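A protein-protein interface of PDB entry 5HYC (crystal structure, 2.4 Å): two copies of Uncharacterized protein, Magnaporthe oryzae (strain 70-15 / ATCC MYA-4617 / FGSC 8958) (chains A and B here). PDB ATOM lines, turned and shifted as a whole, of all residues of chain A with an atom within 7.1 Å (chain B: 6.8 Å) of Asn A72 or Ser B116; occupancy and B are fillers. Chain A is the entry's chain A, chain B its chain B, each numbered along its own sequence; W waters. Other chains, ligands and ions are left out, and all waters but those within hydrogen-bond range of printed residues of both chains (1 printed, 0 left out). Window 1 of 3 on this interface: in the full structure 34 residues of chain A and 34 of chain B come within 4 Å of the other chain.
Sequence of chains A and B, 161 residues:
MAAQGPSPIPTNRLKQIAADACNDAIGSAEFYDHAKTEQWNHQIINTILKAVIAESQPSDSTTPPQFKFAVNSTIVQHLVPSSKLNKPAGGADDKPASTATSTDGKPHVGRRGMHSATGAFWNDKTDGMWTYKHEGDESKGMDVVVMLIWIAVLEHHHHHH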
ATOM      1  N   THR A  37     -17.842  22.540 -25.146  1.00  0.00           N
ATOM      2  CA  THR A  37     -18.893  21.549 -24.948  1.00  0.00           C
ATOM      3  C   THR A  37     -20.240  22.206 -24.748  1.00  0.00           C
ATOM      4  O   THR A  37     -21.275  21.669 -25.144  1.00  0.00           O
ATOM      5  CB  THR A  37     -18.609  20.636 -23.733  1.00  0.00           C
ATOM      6  OG1 THR A  37     -18.205  21.434 -22.622  1.00  0.00           O
ATOM      7  CG2 THR A  37     -17.526  19.622 -24.046  1.00  0.00           C
ATOM      8  N   ASN A  41     -23.378  21.446 -27.075  1.00  0.00           N
ATOM      9  CA  ASN A  41     -24.643  21.028 -26.515  1.00  0.00           C
ATOM     10  C   ASN A  41     -25.785  22.021 -26.823  1.00  0.00           C
ATOM     11  O   ASN A  41     -26.890  21.591 -27.130  1.00  0.00           O
ATOM     12  CB  ASN A  41     -24.488  20.805 -25.002  1.00  0.00           C
ATOM     13  CG  ASN A  41     -24.101  19.360 -24.650  1.00  0.00           C
ATOM     14  OD1 ASN A  41     -24.307  18.441 -25.436  1.00  0.00           O
ATOM     15  ND2 ASN A  41     -23.564  19.165 -23.457  1.00  0.00           N
ATOM     16  N   ILE A  44     -26.707  21.358 -30.436  1.00  0.00           N
ATOM     17  CA  ILE A  44     -27.399  20.097 -30.619  1.00  0.00           C
ATOM     18  C   ILE A  44     -28.841  20.234 -30.143  1.00  0.00           C
ATOM     19  O   ILE A  44     -29.756  19.845 -30.846  1.00  0.00           O
ATOM     20  CB  ILE A  44     -26.699  18.939 -29.851  1.00  0.00           C
ATOM     21  CG1 ILE A  44     -25.396  18.541 -30.549  1.00  0.00           C
ATOM     22  CG2 ILE A  44     -27.623  17.747 -29.697  1.00  0.00           C
ATOM     23  CD1 ILE A  44     -24.412  17.746 -29.641  1.00  0.00           C
ATOM     24  N   ILE A  45     -29.023  20.788 -28.945  1.00  0.00           N
ATOM     25  CA  ILE A  45     -30.344  21.015 -28.370  1.00  0.00           C
ATOM     26  C   ILE A  45     -31.224  21.916 -29.268  1.00  0.00           C
ATOM     27  O   ILE A  45     -32.385  21.610 -29.555  1.00  0.00           O
ATOM     28  CB  ILE A  45     -30.232  21.657 -26.960  1.00  0.00           C
ATOM     29  CG1 ILE A  45     -29.581  20.702 -25.962  1.00  0.00           C
ATOM     30  CG2 ILE A  45     -31.584  22.029 -26.435  1.00  0.00           C
ATOM     31  CD1 ILE A  45     -29.060  21.384 -24.699  1.00  0.00           C
ATOM     32  N   ILE A  48     -32.315  20.154 -32.546  1.00  0.00           N
ATOM     33  CA  ILE A  48     -33.280  19.081 -32.403  1.00  0.00           C
ATOM     34  C   ILE A  48     -34.659  19.633 -32.054  1.00  0.00           C
ATOM     35  O   ILE A  48     -35.647  19.204 -32.628  1.00  0.00           O
ATOM     36  CB  ILE A  48     -32.825  18.036 -31.361  1.00  0.00           C
ATOM     37  CG1 ILE A  48     -31.522  17.386 -31.828  1.00  0.00           C
ATOM     38  CG2 ILE A  48     -33.887  16.967 -31.158  1.00  0.00           C
ATOM     39  CD1 ILE A  48     -30.927  16.359 -30.832  1.00  0.00           C
ATOM     40  N   ALA A  70     -38.703  18.827 -24.376  1.00  0.00           N
ATOM     41  CA  ALA A  70     -37.416  19.062 -23.726  1.00  0.00           C
ATOM     42  C   ALA A  70     -36.341  18.193 -24.365  1.00  0.00           C
ATOM     43  O   ALA A  70     -36.569  17.021 -24.639  1.00  0.00           O
ATOM     44  CB  ALA A  70     -37.503  18.790 -22.219  1.00  0.00           C
ATOM     45  N   VAL A  71     -35.167  18.772 -24.596  1.00  0.00           N
ATOM     46  CA  VAL A  71     -34.039  18.018 -25.116  1.00  0.00           C
ATOM     47  C   VAL A  71     -32.852  18.150 -24.185  1.00  0.00           C
ATOM     48  O   VAL A  71     -32.361  19.251 -23.940  1.00  0.00           O
ATOM     49  CB  VAL A  71     -33.594  18.472 -26.529  1.00  0.00           C
ATOM     50  CG1 VAL A  71     -32.378  17.658 -26.989  1.00  0.00           C
ATOM     51  CG2 VAL A  71     -34.736  18.384 -27.541  1.00  0.00           C
ATOM     52  N   ASN A  72     -32.405  17.013 -23.665  1.00  0.00           N
ATOM     53  CA  ASN A  72     -31.183  16.947 -22.891  1.00  0.00           C
ATOM     54  C   ASN A  72     -30.048  16.312 -23.699  1.00  0.00           C
ATOM     55  O   ASN A  72     -30.198  15.246 -24.275  1.00  0.00           O
ATOM     56  CB  ASN A  72     -31.407  16.164 -21.595  1.00  0.00           C
ATOM     57  CG  ASN A  72     -30.123  15.874 -20.870  1.00  0.00           C
ATOM     58  OD1 ASN A  72     -29.672  14.741 -20.833  1.00  0.00           O
ATOM     59  ND2 ASN A  72     -29.523  16.896 -20.289  1.00  0.00           N
ATOM     60  N   SER A  73     -28.915  16.988 -23.732  1.00  0.00           N
ATOM     61  CA  SER A  73     -27.777  16.525 -24.484  1.00  0.00           C
ATOM     62  C   SER A  73     -26.565  16.436 -23.587  1.00  0.00           C
ATOM     63  O   SER A  73     -26.297  17.346 -22.815  1.00  0.00           O
ATOM     64  CB  SER A  73     -27.499  17.458 -25.660  1.00  0.00           C
ATOM     65  OG  SER A  73     -26.422  16.996 -26.432  1.00  0.00           O
ATOM     66  N   THR A  74     -25.825  15.337 -23.703  1.00  0.00           N
ATOM     67  CA  THR A  74     -24.637  15.119 -22.890  1.00  0.00           C
ATOM     68  C   THR A  74     -23.442  14.792 -23.767  1.00  0.00           C
ATOM     69  O   THR A  74     -23.544  13.967 -24.640  1.00  0.00           O
ATOM     70  CB  THR A  74     -24.829  13.960 -21.890  1.00  0.00           C
ATOM     71  OG1 THR A  74     -25.981  14.196 -21.085  1.00  0.00           O
ATOM     72  CG2 THR A  74     -23.611  13.799 -21.013  1.00  0.00           C
ATOM     73  N   ILE A  75     -22.309  15.427 -23.525  1.00  0.00           N
ATOM     74  CA  ILE A  75     -21.108  15.045 -24.232  1.00  0.00           C
ATOM     75  C   ILE A  75     -20.088  14.467 -23.250  1.00  0.00           C
ATOM     76  O   ILE A  75     -19.789  15.064 -22.227  1.00  0.00           O
ATOM     77  CB  ILE A  75     -20.510  16.229 -25.001  1.00  0.00           C
ATOM     78  CG1 ILE A  75     -21.566  16.811 -25.943  1.00  0.00           C
ATOM     79  CG2 ILE A  75     -19.264  15.798 -25.791  1.00  0.00           C
ATOM     80  CD1 ILE A  75     -21.225  18.131 -26.497  1.00  0.00           C
ATOM     81  N   SER A 116     -27.856   6.250 -16.765  1.00  0.00           N
ATOM     82  CA  SER A 116     -28.848   7.293 -16.768  1.00  0.00           C
ATOM     83  C   SER A 116     -30.217   6.671 -16.927  1.00  0.00           C
ATOM     84  O   SER A 116     -30.460   5.941 -17.868  1.00  0.00           O
ATOM     85  CB  SER A 116     -28.569   8.288 -17.901  1.00  0.00           C
ATOM     86  OG  SER A 116     -29.261   9.505 -17.725  1.00  0.00           O
ATOM     87  N   TYR A 132     -31.069   8.799 -28.061  1.00  0.00           N
ATOM     88  CA  TYR A 132     -30.135   8.542 -29.128  1.00  0.00           C
ATOM     89  C   TYR A 132     -28.695   8.579 -28.603  1.00  0.00           C
ATOM     90  O   TYR A 132     -28.352   9.396 -27.759  1.00  0.00           O
ATOM     91  CB  TYR A 132     -30.343   9.570 -30.240  1.00  0.00           C
ATOM     92  CG  TYR A 132     -29.293   9.502 -31.309  1.00  0.00           C
ATOM     93  CD1 TYR A 132     -29.351   8.543 -32.292  1.00  0.00           C
ATOM     94  CD2 TYR A 132     -28.242  10.398 -31.323  1.00  0.00           C
ATOM     95  CE1 TYR A 132     -28.393   8.472 -33.263  1.00  0.00           C
ATOM     96  CE2 TYR A 132     -27.290  10.344 -32.285  1.00  0.00           C
ATOM     97  CZ  TYR A 132     -27.365   9.378 -33.260  1.00  0.00           C
ATOM     98  OH  TYR A 132     -26.388   9.312 -34.215  1.00  0.00           O
ATOM     99  N   VAL A 145     -24.876  11.679 -26.005  1.00  0.00           N
ATOM    100  CA  VAL A 145     -26.158  11.059 -25.707  1.00  0.00           C
ATOM    101  C   VAL A 145     -27.282  12.096 -25.717  1.00  0.00           C
ATOM    102  O   VAL A 145     -27.151  13.192 -25.192  1.00  0.00           O
ATOM    103  CB  VAL A 145     -26.170  10.341 -24.324  1.00  0.00           C
ATOM    104  CG1 VAL A 145     -27.442   9.549 -24.173  1.00  0.00           C
ATOM    105  CG2 VAL A 145     -24.965   9.399 -24.167  1.00  0.00           C
ATOM    106  N   VAL A 146     -28.411  11.729 -26.292  1.00  0.00           N
ATOM    107  CA  VAL A 146     -29.502  12.652 -26.427  1.00  0.00           C
ATOM    108  C   VAL A 146     -30.803  12.065 -25.889  1.00  0.00           C
ATOM    109  O   VAL A 146     -31.207  10.973 -26.287  1.00  0.00           O
ATOM    110  CB  VAL A 146     -29.688  13.068 -27.921  1.00  0.00           C
ATOM    111  CG1 VAL A 146     -30.952  13.870 -28.097  1.00  0.00           C
ATOM    112  CG2 VAL A 146     -28.471  13.853 -28.428  1.00  0.00           C
ATOM    113  N   MET A 147     -31.454  12.797 -24.986  1.00  0.00           N
ATOM    114  CA  MET A 147     -32.816  12.468 -24.605  1.00  0.00           C
ATOM    115  C   MET A 147     -33.827  13.527 -25.063  1.00  0.00           C
ATOM    116  O   MET A 147     -33.625  14.715 -24.896  1.00  0.00           O
ATOM    117  CB  MET A 147     -32.935  12.283 -23.101  1.00  0.00           C
ATOM    118  CG  MET A 147     -34.357  11.942 -22.671  1.00  0.00           C
ATOM    119  SD  MET A 147     -34.472  11.889 -20.883  1.00  0.00           S
ATOM    120  CE  MET A 147     -34.052  13.572 -20.466  1.00  0.00           C
ATOM    121  N   LEU A 148     -34.921  13.045 -25.637  1.00  0.00           N
ATOM    122  CA  LEU A 148     -36.040  13.864 -26.068  1.00  0.00           C
ATOM    123  C   LEU A 148     -37.269  13.514 -25.274  1.00  0.00           C
ATOM    124  O   LEU A 148     -37.626  12.359 -25.147  1.00  0.00           O
ATOM    125  CB  LEU A 148     -36.308  13.646 -27.549  1.00  0.00           C
ATOM    126  CG  LEU A 148     -37.646  14.127 -28.067  1.00  0.00           C
ATOM    127  CD1 LEU A 148     -37.652  15.658 -28.138  1.00  0.00           C
ATOM    128  CD2 LEU A 148     -37.939  13.504 -29.421  1.00  0.00           C
ATOM    129  N   ILE A 149     -37.919  14.525 -24.730  1.00  0.00           N
ATOM    130  CA  ILE A 149     -39.194  14.334 -24.047  1.00  0.00           C
ATOM    131  C   ILE A 149     -40.304  15.121 -24.760  1.00  0.00           C
ATOM    132  O   ILE A 149     -40.099  16.252 -25.152  1.00  0.00           O
ATOM    133  CB  ILE A 149     -39.090  14.781 -22.582  1.00  0.00           C
ATOM    134  CG1 ILE A 149     -38.040  13.957 -21.837  1.00  0.00           C
ATOM    135  CG2 ILE A 149     -40.424  14.696 -21.901  1.00  0.00           C
ATOM    136  CD1 ILE A 149     -37.796  14.415 -20.417  1.00  0.00           C
ATOM    137  N   ASN B  72     -34.828  12.774 -14.001  1.00  0.00           N
ATOM    138  CA  ASN B  72     -33.721  12.078 -14.631  1.00  0.00           C
ATOM    139  C   ASN B  72     -32.519  11.995 -13.708  1.00  0.00           C
ATOM    140  O   ASN B  72     -32.095  12.994 -13.131  1.00  0.00           O
ATOM    141  CB  ASN B  72     -33.325  12.764 -15.934  1.00  0.00           C
ATOM    142  CG  ASN B  72     -32.154  12.093 -16.600  1.00  0.00           C
ATOM    143  OD1 ASN B  72     -31.002  12.457 -16.378  1.00  0.00           O
ATOM    144  ND2 ASN B  72     -32.438  11.084 -17.401  1.00  0.00           N
ATOM    145  N   THR B  74     -28.491  10.447 -13.295  1.00  0.00           N
ATOM    146  CA  THR B  74     -27.323   9.853 -13.901  1.00  0.00           C
ATOM    147  C   THR B  74     -26.182   9.649 -12.919  1.00  0.00           C
ATOM    148  O   THR B  74     -25.639  10.608 -12.388  1.00  0.00           O
ATOM    149  CB  THR B  74     -26.782  10.710 -15.065  1.00  0.00           C
ATOM    150  OG1 THR B  74     -27.836  11.015 -15.983  1.00  0.00           O
ATOM    151  CG2 THR B  74     -25.676   9.957 -15.779  1.00  0.00           C
ATOM    152  N   MET B 114     -17.143  15.433 -18.913  1.00  0.00           N
ATOM    153  CA  MET B 114     -18.486  15.434 -19.474  1.00  0.00           C
ATOM    154  C   MET B 114     -19.308  16.652 -19.143  1.00  0.00           C
ATOM    155  O   MET B 114     -19.204  17.214 -18.076  1.00  0.00           O
ATOM    156  CB  MET B 114     -19.265  14.185 -19.075  1.00  0.00           C
ATOM    157  CG  MET B 114     -19.523  13.969 -17.632  1.00  0.00           C
ATOM    158  SD  MET B 114     -20.897  12.801 -17.449  1.00  0.00           S
ATOM    159  CE  MET B 114     -22.300  13.892 -17.652  1.00  0.00           C
ATOM    160  N   HIS B 115     -20.124  17.059 -20.104  1.00  0.00           N
ATOM    161  CA  HIS B 115     -20.986  18.222 -19.963  1.00  0.00           C
ATOM    162  C   HIS B 115     -22.403  17.866 -20.354  1.00  0.00           C
ATOM    163  O   HIS B 115     -22.623  17.249 -21.380  1.00  0.00           O
ATOM    164  CB  HIS B 115     -20.478  19.385 -20.819  1.00  0.00           C
ATOM    165  CG  HIS B 115     -21.292  20.635 -20.680  1.00  0.00           C
ATOM    166  ND1 HIS B 115     -22.464  20.844 -21.376  1.00  0.00           N
ATOM    167  CD2 HIS B 115     -21.107  21.736 -19.920  1.00  0.00           C
ATOM    168  CE1 HIS B 115     -22.959  22.023 -21.059  1.00  0.00           C
ATOM    169  NE2 HIS B 115     -22.159  22.584 -20.174  1.00  0.00           N
ATOM    170  N   SER B 116     -23.365  18.248 -19.526  1.00  0.00           N
ATOM    171  CA  SER B 116     -24.762  17.986 -19.820  1.00  0.00           C
ATOM    172  C   SER B 116     -25.572  19.278 -19.758  1.00  0.00           C
ATOM    173  O   SER B 116     -25.356  20.106 -18.884  1.00  0.00           O
ATOM    174  CB  SER B 116     -25.332  16.965 -18.850  1.00  0.00           C
ATOM    175  OG  SER B 116     -26.596  16.517 -19.296  1.00  0.00           O
ATOM    176  N   ALA B 117     -26.501  19.443 -20.691  1.00  0.00           N
ATOM    177  CA  ALA B 117     -27.371  20.609 -20.706  1.00  0.00           C
ATOM    178  C   ALA B 117     -28.750  20.263 -21.240  1.00  0.00           C
ATOM    179  O   ALA B 117     -28.917  19.309 -21.973  1.00  0.00           O
ATOM    180  CB  ALA B 117     -26.754  21.709 -21.517  1.00  0.00           C
ATOM    181  N   THR B 118     -29.742  21.057 -20.859  1.00  0.00           N
ATOM    182  CA  THR B 118     -31.123  20.836 -21.299  1.00  0.00           C
ATOM    183  C   THR B 118     -31.791  22.098 -21.830  1.00  0.00           C
ATOM    184  O   THR B 118     -31.739  23.136 -21.193  1.00  0.00           O
ATOM    185  CB  THR B 118     -31.968  20.289 -20.166  1.00  0.00           C
ATOM    186  OG1 THR B 118     -31.335  19.135 -19.608  1.00  0.00           O
ATOM    187  CG2 THR B 118     -33.341  19.921 -20.660  1.00  0.00           C
ATOM    188  N   GLY B 119     -32.408  21.999 -23.001  1.00  0.00           N
ATOM    189  CA  GLY B 119     -33.226  23.065 -23.556  1.00  0.00           C
ATOM    190  C   GLY B 119     -34.681  22.641 -23.652  1.00  0.00           C
ATOM    191  O   GLY B 119     -34.996  21.474 -23.794  1.00  0.00           O
ATOM    192  N   MET B 129     -37.364  23.654 -14.932  1.00  0.00           N
ATOM    193  CA  MET B 129     -36.485  22.570 -14.574  1.00  0.00           C
ATOM    194  C   MET B 129     -35.508  22.961 -13.494  1.00  0.00           C
ATOM    195  O   MET B 129     -35.176  24.120 -13.319  1.00  0.00           O
ATOM    196  CB  MET B 129     -35.722  22.073 -15.801  1.00  0.00           C
ATOM    197  CG  MET B 129     -35.141  23.194 -16.629  1.00  0.00           C
ATOM    198  SD  MET B 129     -34.290  22.511 -18.033  1.00  0.00           S
ATOM    199  CE  MET B 129     -33.348  21.289 -17.137  1.00  0.00           C
ATOM    200  N   VAL B 145     -25.999  13.094 -10.921  1.00  0.00           N
ATOM    201  CA  VAL B 145     -26.550  14.258 -11.590  1.00  0.00           C
ATOM    202  C   VAL B 145     -28.060  14.077 -11.716  1.00  0.00           C
ATOM    203  O   VAL B 145     -28.544  13.151 -12.343  1.00  0.00           O
ATOM    204  CB  VAL B 145     -25.914  14.471 -12.992  1.00  0.00           C
ATOM    205  CG1 VAL B 145     -26.580  15.625 -13.699  1.00  0.00           C
ATOM    206  CG2 VAL B 145     -24.438  14.745 -12.879  1.00  0.00           C
ATOM    207  N   MET B 147     -31.912  15.736 -12.606  1.00  0.00           N
ATOM    208  CA  MET B 147     -32.724  16.788 -13.184  1.00  0.00           C
ATOM    209  C   MET B 147     -34.209  16.586 -12.925  1.00  0.00           C
ATOM    210  O   MET B 147     -34.740  15.498 -13.112  1.00  0.00           O
ATOM    211  CB  MET B 147     -32.498  16.884 -14.682  1.00  0.00           C
ATOM    212  CG  MET B 147     -33.314  17.980 -15.336  1.00  0.00           C
ATOM    213  SD  MET B 147     -33.221  17.899 -17.124  1.00  0.00           S
ATOM    214  CE  MET B 147     -33.942  16.284 -17.441  1.00  0.00           C
HETATM  215  O   HOH W   1     -26.202  12.646 -18.591  1.00  0.00           O
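ND2 of Asn A41 sits at hydrogen-bond distance from ND1 of His B115, 2.9 Å away. The backbone carbonyl oxygen (O) of Gly B119 is in hydrogen-bond range of the backbone NH (N) of Val A71, 2.8 Å away. The side-chain amide nitrogen (ND2) of Asn A72 lies within hydrogen-bond range of the side-chain hydroxyl (OG) of Ser B116 (3.1 Å). The backbone carbonyl oxygen of Ala B117 sits at hydrogen-bond distance from the side-chain amide nitrogen of Asn A72 (3.0 Å). The side-chain amide nitrogen (ND2) of Asn A72 lies within hydrogen-bond range of the side-chain hydroxyl (OG1) of Thr B118, at 3.0 Å. The backbone NH (N) of Ser A73 sits at hydrogen-bond distance from the backbone carbonyl oxygen (O) of Ala B117. OG of Ser B116 sits at hydrogen-bond distance from OG1 of Thr A74. O of His B115 sits at hydrogen-bond distance from N of Ile A75, at 2.8 Å. The side-chain hydroxyl (OG) of Ser A116 lies within hydrogen-bond range of the side-chain hydroxyl (OG1) of Thr B74 (2.7 Å).
The backbone carbonyl oxygen of Ala A70 is in hydrogen-bond range of the backbone NH of Ile A149 (2.8 Å). O of Asn A72 is in hydrogen-bond range of N of Met A147 (2.8 Å). The backbone carbonyl oxygen (O) of Val A145 is in hydrogen-bond range of the backbone NH (N) of Thr A74. The backbone carbonyl oxygen of Asn B72 is in hydrogen-bond range of the backbone NH of Met B147. The backbone NH of Thr B74 lies within hydrogen-bond range of the backbone carbonyl oxygen of Val B145 (2.9 Å). The side-chain hydroxyl (OG1) of Thr B118 sits at hydrogen-bond distance from the side-chain sulfur (SD) of Met B147 (3.4 Å).
CD1 of Ile A45 touches N of Thr B118, 3.9 Å away. Gly B119 touches Ile A45 (CA to CG2, 3.5 Å). Ala A70 touches Gly B119. Val A71 touches Ala B117 (O to O, 3.97 Å). O of Val A71 touches CA of Thr B118, at 3.3 Å. Ser A73 touches His B115. Ser A73 touches Ser B116 (O to CA, 3.4 Å). CE of Met B114 touches CG2 of Thr A74, 3.6 Å away. His B115 touches Thr A74 (O to CA, 3.3 Å). Ile A75 touches Met B114.
Of the printed residues of chain B, Thr A37 touches His B115 (3.6 Å). Ile A48 touches none of the printed residues of chain B. Asn A72 touches just these residues of chain B: Ser B116, Ala B117 and Thr B118. Of the printed residues of chain B, Thr A74 touches Met B114 (3.6 Å), His B115 (3.3 Å) and Ser B116 (3.0 Å). Of the printed residues of chain A, Asn B72 touches Ser A116 (3.6 Å). Printed residues of chain A within 4 Å of Ser B116: Asn A72 (3.1 Å), Ser A73 (3.4 Å) and Thr A74 (3.0 Å). Met B129 touches none of the printed residues of chain A. The nearest printed residue of chain A that does not touch Ser B116 is Asn A41 (4.01 Å). The nearest printed residue of chain A that does not touch Thr B74 is Thr A74 (6.3 Å).
Of the 18 printed residues of chain A, 10 touch a printed residue of chain B. Hydrophobic or aromatic side chains of chain A within 4 Å of the printed part of chain B: Ile A45 and Ala A70. Among the printed residues, 22 pairs touch across the chains.
Asn A72 touches Ser B116, and with the chains exchanged Ser A116 touches Asn B72. Thr A74 touches Ser B116, and with the chains exchanged Ser A116 touches Thr B74. 5 positions are printed for both chains.
Water W1 lies within hydrogen-bond range of the side-chain hydroxyl of Thr A74 (2.9 Å) and the side-chain hydroxyl of Thr B74 (3.5 Å).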
